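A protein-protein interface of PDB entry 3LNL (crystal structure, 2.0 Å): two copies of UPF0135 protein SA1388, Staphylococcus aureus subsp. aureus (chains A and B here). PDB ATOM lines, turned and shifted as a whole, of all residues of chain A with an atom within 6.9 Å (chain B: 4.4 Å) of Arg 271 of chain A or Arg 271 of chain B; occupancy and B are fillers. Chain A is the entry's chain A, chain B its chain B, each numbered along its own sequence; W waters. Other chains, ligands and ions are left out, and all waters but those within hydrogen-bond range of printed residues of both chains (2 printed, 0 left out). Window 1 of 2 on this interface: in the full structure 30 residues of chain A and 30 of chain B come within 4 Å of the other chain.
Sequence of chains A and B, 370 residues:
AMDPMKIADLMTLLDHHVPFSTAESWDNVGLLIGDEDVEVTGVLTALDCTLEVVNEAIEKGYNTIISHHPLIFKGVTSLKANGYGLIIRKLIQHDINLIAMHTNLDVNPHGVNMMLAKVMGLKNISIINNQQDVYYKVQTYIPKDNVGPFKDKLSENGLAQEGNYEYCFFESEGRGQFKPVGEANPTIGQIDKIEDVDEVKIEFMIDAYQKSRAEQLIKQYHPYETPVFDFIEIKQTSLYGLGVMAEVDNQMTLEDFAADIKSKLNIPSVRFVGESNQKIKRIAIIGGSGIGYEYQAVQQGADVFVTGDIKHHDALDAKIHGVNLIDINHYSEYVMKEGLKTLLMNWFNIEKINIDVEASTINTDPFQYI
The side-chain amide oxygen (OD1) of Asn 329 of chain A is in hydrogen-bond range of the guanidinium group (NH1) of Arg 271 of chain B, 3.5 Å away.
The side-chain hydroxyl of Tyr 369 of chain B sits at hydrogen-bond distance from the guanidinium group of Arg 271 of chain A.
The guanidinium group (NH2) of Arg 271 of chain A sits close to the guanidinium group (NH2) of Arg 271 of chain B.
N of Ile 370 of chain A sits at hydrogen-bond distance from O of Val 270 of chain B.
OH of Tyr 369 of chain A sits at hydrogen-bond distance from NH1 of Arg 271 of chain B.
N of Phe 272 of chain B lies within hydrogen-bond range of O of Gln 368 of chain A, 2.8 Å away.
The backbone NH of Phe 272 of chain A sits at hydrogen-bond distance from the backbone carbonyl oxygen of Gln 368 of chain B.
The guanidinium group of Arg 271 of chain B is in salt-bridge range of the side-chain carboxylate of Asp 327 of chain B (3.1 Å).
OD1 of Asp 327 of chain A is in hydrogen-bond range of N of Asn 329 of chain A, 2.8 Å away.
The backbone carbonyl oxygen of Ser 269 of chain A sits at hydrogen-bond distance from the side-chain amide nitrogen of Asn 329 of chain A, 2.9 Å away.
The backbone carbonyl oxygen (O) of Ile 310 of chain A is in hydrogen-bond range of the guanidinium group (NH2) of Arg 271 of chain A.
N of Val 273 of chain A sits at hydrogen-bond distance from O of Leu 325 of chain A, 2.8 Å away.
The guanidinium group (NE) of Arg 271 of chain A lies within salt-bridge range of the side-chain carboxylate (OD2) of Asp 327 of chain A, 3.1 Å away.
Tyr 369 of chain B touches Ser 269 of chain A.
Val 270 of chain A touches Tyr 369 of chain B (O to CA, 3.5 Å).
NH1 of Arg 271 of chain A touches OD1 of Asn 329 of chain B, at 3.6 Å.
O of Gln 368 of chain B touches CA of Arg 271 of chain A (3.2 Å).
O of Phe 272 of chain A touches CA of Phe 367 of chain B, at 3.4 Å.
Ile 310 of chain A touches Phe 367 of chain B (O to CZ, 3.5 Å).
Arg 271 of chain B touches Phe 367 of chain A.
Phe 272 of chain B touches Phe 367 of chain A (O to CA, 3.5 Å).
Ile 310 of chain B touches Phe 367 of chain A (O to CZ, 3.5 Å).
Phe 272 of chain B touches Ile 370 of chain A (CE2 to CG2, 3.9 Å).
Arg 271 of chain A touches just these residues of chain B: Arg 271 (3.5 Å), Asn 329 (3.6 Å), Phe 367 (3.6 Å), Gln 368 (3.2 Å) and Tyr 369 (3.0 Å).
Printed residues of chain B within 4 Å of Phe 272 of chain A: Phe 367 and Gln 368.
Printed residues of chain B within 4 Å of Ile 310 of chain A: Phe 367 (3.5 Å).
His 330 of chain A touches none of the printed residues of chain B.
Of the printed residues of chain B, Tyr 369 of chain A touches Val 270 (3.5 Å) and Arg 271 (3.0 Å).
Printed residues of chain A within 4 Å of Val 270 of chain B: Tyr 369 (3.5 Å) and Ile 370 (2.9 Å).
Of the printed residues of chain A, Tyr 369 of chain B touches Ser 269, Val 270 and Arg 271.
The nearest residue of chain A that does not touch Arg 271 of chain B is Ile 370 of chain A (4.9 Å).
Hydrophobic or aromatic side chains of chain B within 4 Å of the printed part of chain A: Phe 272, Ile 310, Phe 367 and Tyr 369.
Of the 22 printed residues of chain A, 11 touch a printed residue of chain B.
Among the printed residues, 21 pairs touch across the chains.
Among the printed residues, no Asp or Glu carboxylate lies within 4 Å of a Lys or Arg side-chain nitrogen of the other chain.
Arg 271 of chain A touches Asn 329 of chain B, and with the chains exchanged Asn 329 of chain A touches Arg 271 of chain B.
Arg 271 of chain A touches Gln 368 of chain B, and with the chains exchanged Gln 368 of chain A touches Arg 271 of chain B.
Arg 271 of chain A touches Tyr 369 of chain B, and with the chains exchanged Tyr 369 of chain A touches Arg 271 of chain B.
Phe 272 of chain A touches Phe 367 of chain B, and with the chains exchanged Phe 367 of chain A touches Phe 272 of chain B.
Of the 21 pairs that touch across the chains among the printed residues, 17 have their exchanged pair printed and touching as well.
Water W2 lies within hydrogen-bond range of OD1 of Asn 329 of chain A (2.7 Å), OD2 of Asp 327 of chain A (2.9 Å) and NH1 of Arg 271 of chain B (2.9 Å).
Water W1 lies within hydrogen-bond range of OD1 of Asn 329 of chain B, OD2 of Asp 327 of chain B and NH1 of Arg 271 of chain A.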
ATOM      1  N   ALA A 258      12.581  17.350  27.171  1.00  0.00           N
ATOM      2  CA  ALA A 258      13.773  16.533  26.929  1.00  0.00           C
ATOM      3  C   ALA A 258      14.872  16.844  27.934  1.00  0.00           C
ATOM      4  O   ALA A 258      15.493  15.975  28.484  1.00  0.00           O
ATOM      5  CB  ALA A 258      14.286  16.736  25.531  1.00  0.00           C
ATOM      6  N   SER A 269      23.566  12.487  27.474  1.00  0.00           N
ATOM      7  CA  SER A 269      23.159  13.032  26.184  1.00  0.00           C
ATOM      8  C   SER A 269      21.784  12.518  25.853  1.00  0.00           C
ATOM      9  O   SER A 269      21.539  11.329  25.928  1.00  0.00           O
ATOM     10  CB  SER A 269      24.111  12.594  25.083  1.00  0.00           C
ATOM     11  OG  SER A 269      23.749  13.219  23.873  1.00  0.00           O
ATOM     12  N   VAL A 270      20.886  13.426  25.525  1.00  0.00           N
ATOM     13  CA  VAL A 270      19.592  13.095  24.951  1.00  0.00           C
ATOM     14  C   VAL A 270      19.452  13.759  23.602  1.00  0.00           C
ATOM     15  O   VAL A 270      20.066  14.841  23.303  1.00  0.00           O
ATOM     16  CB  VAL A 270      18.523  13.541  25.978  1.00  0.00           C
ATOM     17  CG1 VAL A 270      17.141  13.675  25.455  1.00  0.00           C
ATOM     18  CG2 VAL A 270      18.567  12.582  27.169  1.00  0.00           C
ATOM     19  N   ARG A 271      18.630  13.158  22.763  1.00  0.00           N
ATOM     20  CA  ARG A 271      18.310  13.734  21.458  1.00  0.00           C
ATOM     21  C   ARG A 271      16.820  13.642  21.178  1.00  0.00           C
ATOM     22  O   ARG A 271      16.178  12.672  21.572  1.00  0.00           O
ATOM     23  CB  ARG A 271      19.099  13.079  20.318  1.00  0.00           C
ATOM     24  CG  ARG A 271      19.001  11.584  20.251  1.00  0.00           C
ATOM     25  CD  ARG A 271      20.077  11.025  19.365  1.00  0.00           C
ATOM     26  NE  ARG A 271      20.017   9.575  19.264  1.00  0.00           N
ATOM     27  CZ  ARG A 271      20.928   8.833  18.628  1.00  0.00           C
ATOM     28  NH1 ARG A 271      21.980   9.391  18.066  1.00  0.00           N
ATOM     29  NH2 ARG A 271      20.820   7.521  18.599  1.00  0.00           N
ATOM     30  N   PHE A 272      16.270  14.665  20.520  1.00  0.00           N
ATOM     31  CA  PHE A 272      14.870  14.680  20.206  1.00  0.00           C
ATOM     32  C   PHE A 272      14.601  14.985  18.717  1.00  0.00           C
ATOM     33  O   PHE A 272      15.420  15.537  18.008  1.00  0.00           O
ATOM     34  CB  PHE A 272      14.073  15.607  21.136  1.00  0.00           C
ATOM     35  CG  PHE A 272      14.395  17.065  20.997  1.00  0.00           C
ATOM     36  CD1 PHE A 272      13.712  17.881  20.131  1.00  0.00           C
ATOM     37  CD2 PHE A 272      15.340  17.653  21.815  1.00  0.00           C
ATOM     38  CE1 PHE A 272      14.022  19.213  20.030  1.00  0.00           C
ATOM     39  CE2 PHE A 272      15.625  18.980  21.738  1.00  0.00           C
ATOM     40  CZ  PHE A 272      14.979  19.779  20.908  1.00  0.00           C
ATOM     41  N   VAL A 273      13.429  14.588  18.293  1.00  0.00           N
ATOM     42  CA  VAL A 273      12.941  14.763  16.926  1.00  0.00           C
ATOM     43  C   VAL A 273      11.653  15.565  17.015  1.00  0.00           C
ATOM     44  O   VAL A 273      10.680  15.165  17.674  1.00  0.00           O
ATOM     45  CB  VAL A 273      12.671  13.439  16.230  1.00  0.00           C
ATOM     46  CG1 VAL A 273      12.140  13.678  14.702  1.00  0.00           C
ATOM     47  CG2 VAL A 273      13.920  12.481  16.313  1.00  0.00           C
ATOM     48  N   THR A 307      11.702   6.702  23.894  1.00  0.00           N
ATOM     49  CA  THR A 307      12.268   5.358  23.856  1.00  0.00           C
ATOM     50  C   THR A 307      13.794   5.463  23.747  1.00  0.00           C
ATOM     51  O   THR A 307      14.361   6.556  23.895  1.00  0.00           O
ATOM     52  CB  THR A 307      11.663   4.492  22.718  1.00  0.00           C
ATOM     53  OG1 THR A 307      11.968   3.110  22.949  1.00  0.00           O
ATOM     54  CG2 THR A 307      12.163   4.913  21.314  1.00  0.00           C
ATOM     55  N   GLY A 308      14.471   4.347  23.514  1.00  0.00           N
ATOM     56  CA  GLY A 308      15.915   4.366  23.245  1.00  0.00           C
ATOM     57  C   GLY A 308      16.264   3.802  21.883  1.00  0.00           C
ATOM     58  O   GLY A 308      15.386   3.227  21.163  1.00  0.00           O
ATOM     59  N   ASP A 309      17.547   3.856  21.557  1.00  0.00           N
ATOM     60  CA  ASP A 309      18.111   3.150  20.380  1.00  0.00           C
ATOM     61  C   ASP A 309      17.409   3.647  19.100  1.00  0.00           C
ATOM     62  O   ASP A 309      17.146   2.853  18.204  1.00  0.00           O
ATOM     63  CB  ASP A 309      17.891   1.620  20.466  1.00  0.00           C
ATOM     64  CG  ASP A 309      18.983   0.842  21.244  1.00  0.00           C
ATOM     65  OD1 ASP A 309      20.040   1.410  21.594  1.00  0.00           O
ATOM     66  OD2 ASP A 309      18.760  -0.386  21.500  1.00  0.00           O
ATOM     67  N   ILE A 310      17.133   4.949  19.000  1.00  0.00           N
ATOM     68  CA  ILE A 310      16.520   5.479  17.794  1.00  0.00           C
ATOM     69  C   ILE A 310      17.576   5.684  16.704  1.00  0.00           C
ATOM     70  O   ILE A 310      18.632   6.269  16.960  1.00  0.00           O
ATOM     71  CB  ILE A 310      15.742   6.785  18.048  1.00  0.00           C
ATOM     72  CG1 ILE A 310      14.835   6.621  19.282  1.00  0.00           C
ATOM     73  CG2 ILE A 310      14.934   7.181  16.748  1.00  0.00           C
ATOM     74  CD1 ILE A 310      13.947   7.822  19.574  1.00  0.00           C
ATOM     75  N   LYS A 311      17.293   5.160  15.507  1.00  0.00           N
ATOM     76  CA  LYS A 311      18.192   5.296  14.403  1.00  0.00           C
ATOM     77  C   LYS A 311      17.748   6.350  13.402  1.00  0.00           C
ATOM     78  O   LYS A 311      16.588   6.780  13.422  1.00  0.00           O
ATOM     79  CB  LYS A 311      18.351   3.959  13.715  1.00  0.00           C
ATOM     80  CG  LYS A 311      19.059   2.911  14.603  1.00  0.00           C
ATOM     81  CD  LYS A 311      19.332   1.608  13.855  1.00  0.00           C
ATOM     82  CE  LYS A 311      18.067   1.036  13.260  1.00  0.00           C
ATOM     83  NZ  LYS A 311      18.465  -0.154  12.391  1.00  0.00           N
ATOM     84  N   HIS A 312      18.707   6.784  12.571  1.00  0.00           N
ATOM     85  CA  HIS A 312      18.531   7.915  11.648  1.00  0.00           C
ATOM     86  C   HIS A 312      17.266   7.832  10.817  1.00  0.00           C
ATOM     87  O   HIS A 312      16.510   8.778  10.776  1.00  0.00           O
ATOM     88  CB  HIS A 312      19.735   8.049  10.730  1.00  0.00           C
ATOM     89  CG  HIS A 312      19.576   9.072   9.649  1.00  0.00           C
ATOM     90  ND1 HIS A 312      19.761  10.409   9.879  1.00  0.00           N
ATOM     91  CD2 HIS A 312      19.305   8.948   8.326  1.00  0.00           C
ATOM     92  CE1 HIS A 312      19.526  11.078   8.766  1.00  0.00           C
ATOM     93  NE2 HIS A 312      19.287  10.212   7.794  1.00  0.00           N
ATOM     94  N   LEU A 325       9.672  12.535  18.819  1.00  0.00           N
ATOM     95  CA  LEU A 325      10.396  11.502  19.559  1.00  0.00           C
ATOM     96  C   LEU A 325      11.407  12.090  20.506  1.00  0.00           C
ATOM     97  O   LEU A 325      11.982  13.182  20.269  1.00  0.00           O
ATOM     98  CB  LEU A 325      11.214  10.603  18.607  1.00  0.00           C
ATOM     99  CG  LEU A 325      10.542  10.027  17.372  1.00  0.00           C
ATOM    100  CD1 LEU A 325      11.582   9.278  16.502  1.00  0.00           C
ATOM    101  CD2 LEU A 325       9.399   9.104  17.770  1.00  0.00           C
ATOM    102  N   ILE A 326      11.724  11.296  21.509  1.00  0.00           N
ATOM    103  CA  ILE A 326      12.881  11.546  22.329  1.00  0.00           C
ATOM    104  C   ILE A 326      13.612  10.226  22.530  1.00  0.00           C
ATOM    105  O   ILE A 326      12.998   9.205  22.879  1.00  0.00           O
ATOM    106  CB  ILE A 326      12.528  12.154  23.690  1.00  0.00           C
ATOM    107  CG1 ILE A 326      11.788  13.507  23.568  1.00  0.00           C
ATOM    108  CG2 ILE A 326      13.823  12.344  24.528  1.00  0.00           C
ATOM    109  CD1 ILE A 326      11.157  14.031  24.961  1.00  0.00           C
ATOM    110  N   ASP A 327      14.914  10.249  22.252  1.00  0.00           N
ATOM    111  CA  ASP A 327      15.809   9.138  22.538  1.00  0.00           C
ATOM    112  C   ASP A 327      16.478   9.423  23.869  1.00  0.00           C
ATOM    113  O   ASP A 327      17.395  10.255  23.950  1.00  0.00           O
ATOM    114  CB  ASP A 327      16.843   8.948  21.428  1.00  0.00           C
ATOM    115  CG  ASP A 327      17.641   7.640  21.544  1.00  0.00           C
ATOM    116  OD1 ASP A 327      17.568   6.978  22.597  1.00  0.00           O
ATOM    117  OD2 ASP A 327      18.378   7.321  20.571  1.00  0.00           O
ATOM    118  N   ILE A 328      16.010   8.716  24.914  1.00  0.00           N
ATOM    119  CA  ILE A 328      16.618   8.762  26.232  1.00  0.00           C
ATOM    120  C   ILE A 328      17.699   7.671  26.451  1.00  0.00           C
ATOM    121  O   ILE A 328      18.245   7.552  27.574  1.00  0.00           O
ATOM    122  CB  ILE A 328      15.560   8.651  27.375  1.00  0.00           C
ATOM    123  CG1 ILE A 328      14.751   7.332  27.291  1.00  0.00           C
ATOM    124  CG2 ILE A 328      14.666   9.964  27.359  1.00  0.00           C
ATOM    125  CD1 ILE A 328      13.772   7.014  28.510  1.00  0.00           C
ATOM    126  N   ASN A 329      17.998   6.939  25.374  1.00  0.00           N
ATOM    127  CA  ASN A 329      18.936   5.811  25.328  1.00  0.00           C
ATOM    128  C   ASN A 329      18.292   4.554  25.936  1.00  0.00           C
ATOM    129  O   ASN A 329      17.495   4.621  26.884  1.00  0.00           O
ATOM    130  CB  ASN A 329      20.281   6.159  25.914  1.00  0.00           C
ATOM    131  CG  ASN A 329      20.856   7.427  25.284  1.00  0.00           C
ATOM    132  OD1 ASN A 329      20.868   7.543  24.055  1.00  0.00           O
ATOM    133  ND2 ASN A 329      21.276   8.399  26.101  1.00  0.00           N
ATOM    134  N   HIS A 330      18.594   3.427  25.323  1.00  0.00           N
ATOM    135  CA  HIS A 330      18.193   2.122  25.841  1.00  0.00           C
ATOM    136  C   HIS A 330      18.655   1.992  27.280  1.00  0.00           C
ATOM    137  O   HIS A 330      17.931   1.483  28.114  1.00  0.00           O
ATOM    138  CB  HIS A 330      18.852   1.076  24.965  1.00  0.00           C
ATOM    139  CG  HIS A 330      18.321  -0.331  25.131  1.00  0.00           C
ATOM    140  ND1 HIS A 330      18.053  -1.145  24.051  1.00  0.00           N
ATOM    141  CD2 HIS A 330      17.986  -1.040  26.223  1.00  0.00           C
ATOM    142  CE1 HIS A 330      17.626  -2.322  24.485  1.00  0.00           C
ATOM    143  NE2 HIS A 330      17.497  -2.257  25.792  1.00  0.00           N
ATOM    144  N   PHE A 367      28.488   2.424  26.528  1.00  0.00           N
ATOM    145  CA  PHE A 367      28.808   3.697  25.986  1.00  0.00           C
ATOM    146  C   PHE A 367      29.356   4.649  27.013  1.00  0.00           C
ATOM    147  O   PHE A 367      28.806   4.800  28.116  1.00  0.00           O
ATOM    148  CB  PHE A 367      27.581   4.378  25.383  1.00  0.00           C
ATOM    149  CG  PHE A 367      27.077   3.777  24.102  1.00  0.00           C
ATOM    150  CD1 PHE A 367      25.715   3.437  23.981  1.00  0.00           C
ATOM    151  CD2 PHE A 367      27.901   3.671  22.997  1.00  0.00           C
ATOM    152  CE1 PHE A 367      25.195   2.916  22.832  1.00  0.00           C
ATOM    153  CE2 PHE A 367      27.398   3.139  21.814  1.00  0.00           C
ATOM    154  CZ  PHE A 367      26.030   2.753  21.729  1.00  0.00           C
ATOM    155  N   GLN A 368      30.405   5.359  26.589  1.00  0.00           N
ATOM    156  CA  GLN A 368      30.882   6.574  27.243  1.00  0.00           C
ATOM    157  C   GLN A 368      30.711   7.762  26.283  1.00  0.00           C
ATOM    158  O   GLN A 368      31.134   7.707  25.113  1.00  0.00           O
ATOM    159  CB  GLN A 368      32.365   6.379  27.620  1.00  0.00           C
ATOM    160  CG  GLN A 368      32.938   7.604  28.298  1.00  0.00           C
ATOM    161  CD  GLN A 368      34.247   7.358  29.037  1.00  0.00           C
ATOM    162  OE1 GLN A 368      34.700   6.206  29.227  1.00  0.00           O
ATOM    163  NE2 GLN A 368      34.872   8.462  29.451  1.00  0.00           N
ATOM    164  N   TYR A 369      30.129   8.844  26.794  1.00  0.00           N
ATOM    165  CA  TYR A 369      29.755   9.979  26.028  1.00  0.00           C
ATOM    166  C   TYR A 369      30.722  11.130  26.166  1.00  0.00           C
ATOM    167  O   TYR A 369      31.259  11.383  27.228  1.00  0.00           O
ATOM    168  CB  TYR A 369      28.386  10.494  26.461  1.00  0.00           C
ATOM    169  CG  TYR A 369      27.280   9.592  26.074  1.00  0.00           C
ATOM    170  CD1 TYR A 369      26.994   8.437  26.828  1.00  0.00           C
ATOM    171  CD2 TYR A 369      26.505   9.872  24.987  1.00  0.00           C
ATOM    172  CE1 TYR A 369      25.918   7.582  26.474  1.00  0.00           C
ATOM    173  CE2 TYR A 369      25.449   9.035  24.610  1.00  0.00           C
ATOM    174  CZ  TYR A 369      25.202   7.853  25.302  1.00  0.00           C
ATOM    175  OH  TYR A 369      24.149   7.042  24.861  1.00  0.00           O
ATOM    176  N   ILE A 370      30.957  11.833  25.072  1.00  0.00           N
ATOM    177  CA  ILE A 370      31.809  12.979  25.085  1.00  0.00           C
ATOM    178  C   ILE A 370      31.263  14.090  24.222  1.00  0.00           C
ATOM    179  O   ILE A 370      30.305  13.939  23.460  1.00  0.00           O
ATOM    180  CB  ILE A 370      33.255  12.660  24.639  1.00  0.00           C
ATOM    181  CG1 ILE A 370      33.304  12.114  23.208  1.00  0.00           C
ATOM    182  CG2 ILE A 370      33.969  11.765  25.688  1.00  0.00           C
ATOM    183  CD1 ILE A 370      34.725  12.030  22.662  1.00  0.00           C
ATOM    184  OXT ILE A 370      31.828  15.197  24.301  1.00  0.00           O
ATOM    185  N   VAL B 270      29.252  12.523  20.723  1.00  0.00           N
ATOM    186  CA  VAL B 270      29.842  11.271  20.301  1.00  0.00           C
ATOM    187  C   VAL B 270      29.862  10.312  21.492  1.00  0.00           C
ATOM    188  O   VAL B 270      29.920  10.763  22.635  1.00  0.00           O
ATOM    189  CB  VAL B 270      31.259  11.559  19.726  1.00  0.00           C
ATOM    190  CG1 VAL B 270      32.111  10.334  19.657  1.00  0.00           C
ATOM    191  CG2 VAL B 270      31.089  12.256  18.315  1.00  0.00           C
ATOM    192  N   ARG B 271      29.759   9.013  21.216  1.00  0.00           N
ATOM    193  CA  ARG B 271      29.929   7.994  22.243  1.00  0.00           C
ATOM    194  C   ARG B 271      30.844   6.874  21.758  1.00  0.00           C
ATOM    195  O   ARG B 271      30.896   6.532  20.542  1.00  0.00           O
ATOM    196  CB  ARG B 271      28.559   7.436  22.701  1.00  0.00           C
ATOM    197  CG  ARG B 271      27.709   6.883  21.607  1.00  0.00           C
ATOM    198  CD  ARG B 271      26.242   6.729  22.018  1.00  0.00           C
ATOM    199  NE  ARG B 271      25.420   6.275  20.883  1.00  0.00           N
ATOM    200  CZ  ARG B 271      24.099   6.116  20.921  1.00  0.00           C
ATOM    201  NH1 ARG B 271      23.418   6.386  22.029  1.00  0.00           N
ATOM    202  NH2 ARG B 271      23.445   5.645  19.856  1.00  0.00           N
ATOM    203  N   PHE B 272      31.602   6.310  22.697  1.00  0.00           N
ATOM    204  CA  PHE B 272      32.533   5.294  22.354  1.00  0.00           C
ATOM    205  C   PHE B 272      32.416   4.124  23.285  1.00  0.00           C
ATOM    206  O   PHE B 272      31.826   4.217  24.345  1.00  0.00           O
ATOM    207  CB  PHE B 272      33.957   5.833  22.255  1.00  0.00           C
ATOM    208  CG  PHE B 272      34.547   6.309  23.547  1.00  0.00           C
ATOM    209  CD1 PHE B 272      35.224   5.440  24.380  1.00  0.00           C
ATOM    210  CD2 PHE B 272      34.506   7.650  23.884  1.00  0.00           C
ATOM    211  CE1 PHE B 272      35.781   5.907  25.563  1.00  0.00           C
ATOM    212  CE2 PHE B 272      35.102   8.114  25.035  1.00  0.00           C
ATOM    213  CZ  PHE B 272      35.718   7.235  25.878  1.00  0.00           C
ATOM    214  N   ILE B 310      24.736   3.033  16.484  1.00  0.00           N
ATOM    215  CA  ILE B 310      25.091   1.892  17.342  1.00  0.00           C
ATOM    216  C   ILE B 310      24.041   1.745  18.451  1.00  0.00           C
ATOM    217  O   ILE B 310      23.653   2.735  19.104  1.00  0.00           O
ATOM    218  CB  ILE B 310      26.495   2.011  17.934  1.00  0.00           C
ATOM    219  CG1 ILE B 310      27.509   2.296  16.800  1.00  0.00           C
ATOM    220  CG2 ILE B 310      26.830   0.730  18.705  1.00  0.00           C
ATOM    221  CD1 ILE B 310      28.975   2.390  17.206  1.00  0.00           C
ATOM    222  N   ILE B 326      33.377   3.603  17.984  1.00  0.00           N
ATOM    223  CA  ILE B 326      32.926   4.982  18.087  1.00  0.00           C
ATOM    224  C   ILE B 326      31.679   5.165  17.214  1.00  0.00           C
ATOM    225  O   ILE B 326      31.667   4.874  16.011  1.00  0.00           O
ATOM    226  CB  ILE B 326      34.003   6.061  17.695  1.00  0.00           C
ATOM    227  CG1 ILE B 326      35.282   5.884  18.503  1.00  0.00           C
ATOM    228  CG2 ILE B 326      33.431   7.468  17.930  1.00  0.00           C
ATOM    229  CD1 ILE B 326      36.483   6.637  18.027  1.00  0.00           C
ATOM    230  N   ASP B 327      30.625   5.674  17.842  1.00  0.00           N
ATOM    231  CA  ASP B 327      29.435   6.154  17.166  1.00  0.00           C
ATOM    232  C   ASP B 327      29.586   7.625  16.860  1.00  0.00           C
ATOM    233  O   ASP B 327      29.444   8.471  17.735  1.00  0.00           O
ATOM    234  CB  ASP B 327      28.210   5.902  18.042  1.00  0.00           C
ATOM    235  CG  ASP B 327      26.878   6.055  17.309  1.00  0.00           C
ATOM    236  OD1 ASP B 327      26.845   6.642  16.205  1.00  0.00           O
ATOM    237  OD2 ASP B 327      25.857   5.581  17.871  1.00  0.00           O
ATOM    238  N   ASN B 329      27.521   8.971  14.749  1.00  0.00           N
ATOM    239  CA  ASN B 329      26.163   9.176  14.251  1.00  0.00           C
ATOM    240  C   ASN B 329      26.075   8.927  12.753  1.00  0.00           C
ATOM    241  O   ASN B 329      27.057   9.095  12.000  1.00  0.00           O
ATOM    242  CB  ASN B 329      25.606  10.544  14.681  1.00  0.00           C
ATOM    243  CG  ASN B 329      25.680  10.751  16.206  1.00  0.00           C
ATOM    244  OD1 ASN B 329      25.367   9.833  16.972  1.00  0.00           O
ATOM    245  ND2 ASN B 329      26.205  11.905  16.633  1.00  0.00           N
ATOM    246  N   PHE B 367      17.602  14.566  14.408  1.00  0.00           N
ATOM    247  CA  PHE B 367      17.910  14.695  15.776  1.00  0.00           C
ATOM    248  C   PHE B 367      18.399  16.117  16.098  1.00  0.00           C
ATOM    249  O   PHE B 367      19.201  16.679  15.374  1.00  0.00           O
ATOM    250  CB  PHE B 367      18.995  13.712  16.189  1.00  0.00           C
ATOM    251  CG  PHE B 367      18.563  12.296  16.225  1.00  0.00           C
ATOM    252  CD1 PHE B 367      19.315  11.316  15.593  1.00  0.00           C
ATOM    253  CD2 PHE B 367      17.453  11.913  16.974  1.00  0.00           C
ATOM    254  CE1 PHE B 367      18.935   9.997  15.672  1.00  0.00           C
ATOM    255  CE2 PHE B 367      17.076  10.593  17.058  1.00  0.00           C
ATOM    256  CZ  PHE B 367      17.832   9.625  16.402  1.00  0.00           C
ATOM    257  N   GLN B 368      17.887  16.648  17.208  1.00  0.00           N
ATOM    258  CA  GLN B 368      18.520  17.746  17.951  1.00  0.00           C
ATOM    259  C   GLN B 368      18.998  17.238  19.329  1.00  0.00           C
ATOM    260  O   GLN B 368      18.263  16.580  20.069  1.00  0.00           O
ATOM    261  CB  GLN B 368      17.533  18.918  18.031  1.00  0.00           C
ATOM    262  CG  GLN B 368      18.007  20.054  18.875  1.00  0.00           C
ATOM    263  CD  GLN B 368      17.103  21.293  18.797  1.00  0.00           C
ATOM    264  OE1 GLN B 368      16.258  21.455  17.882  1.00  0.00           O
ATOM    265  NE2 GLN B 368      17.285  22.173  19.788  1.00  0.00           N
ATOM    266  N   TYR B 369      20.258  17.544  19.653  1.00  0.00           N
ATOM    267  CA  TYR B 369      20.940  17.097  20.831  1.00  0.00           C
ATOM    268  C   TYR B 369      20.926  18.118  21.933  1.00  0.00           C
ATOM    269  O   TYR B 369      21.042  19.313  21.669  1.00  0.00           O
ATOM    270  CB  TYR B 369      22.400  16.777  20.518  1.00  0.00           C
ATOM    271  CG  TYR B 369      22.555  15.563  19.655  1.00  0.00           C
ATOM    272  CD1 TYR B 369      22.301  15.632  18.280  1.00  0.00           C
ATOM    273  CD2 TYR B 369      22.839  14.332  20.213  1.00  0.00           C
ATOM    274  CE1 TYR B 369      22.447  14.544  17.477  1.00  0.00           C
ATOM    275  CE2 TYR B 369      22.948  13.209  19.433  1.00  0.00           C
ATOM    276  CZ  TYR B 369      22.754  13.313  18.060  1.00  0.00           C
ATOM    277  OH  TYR B 369      22.826  12.203  17.260  1.00  0.00           O
HETATM  278  O   HOH W   1      23.864   7.436  16.824  1.00  0.00           O
HETATM  279  O   HOH W   2      20.537   5.961  21.904  1.00  0.00           O
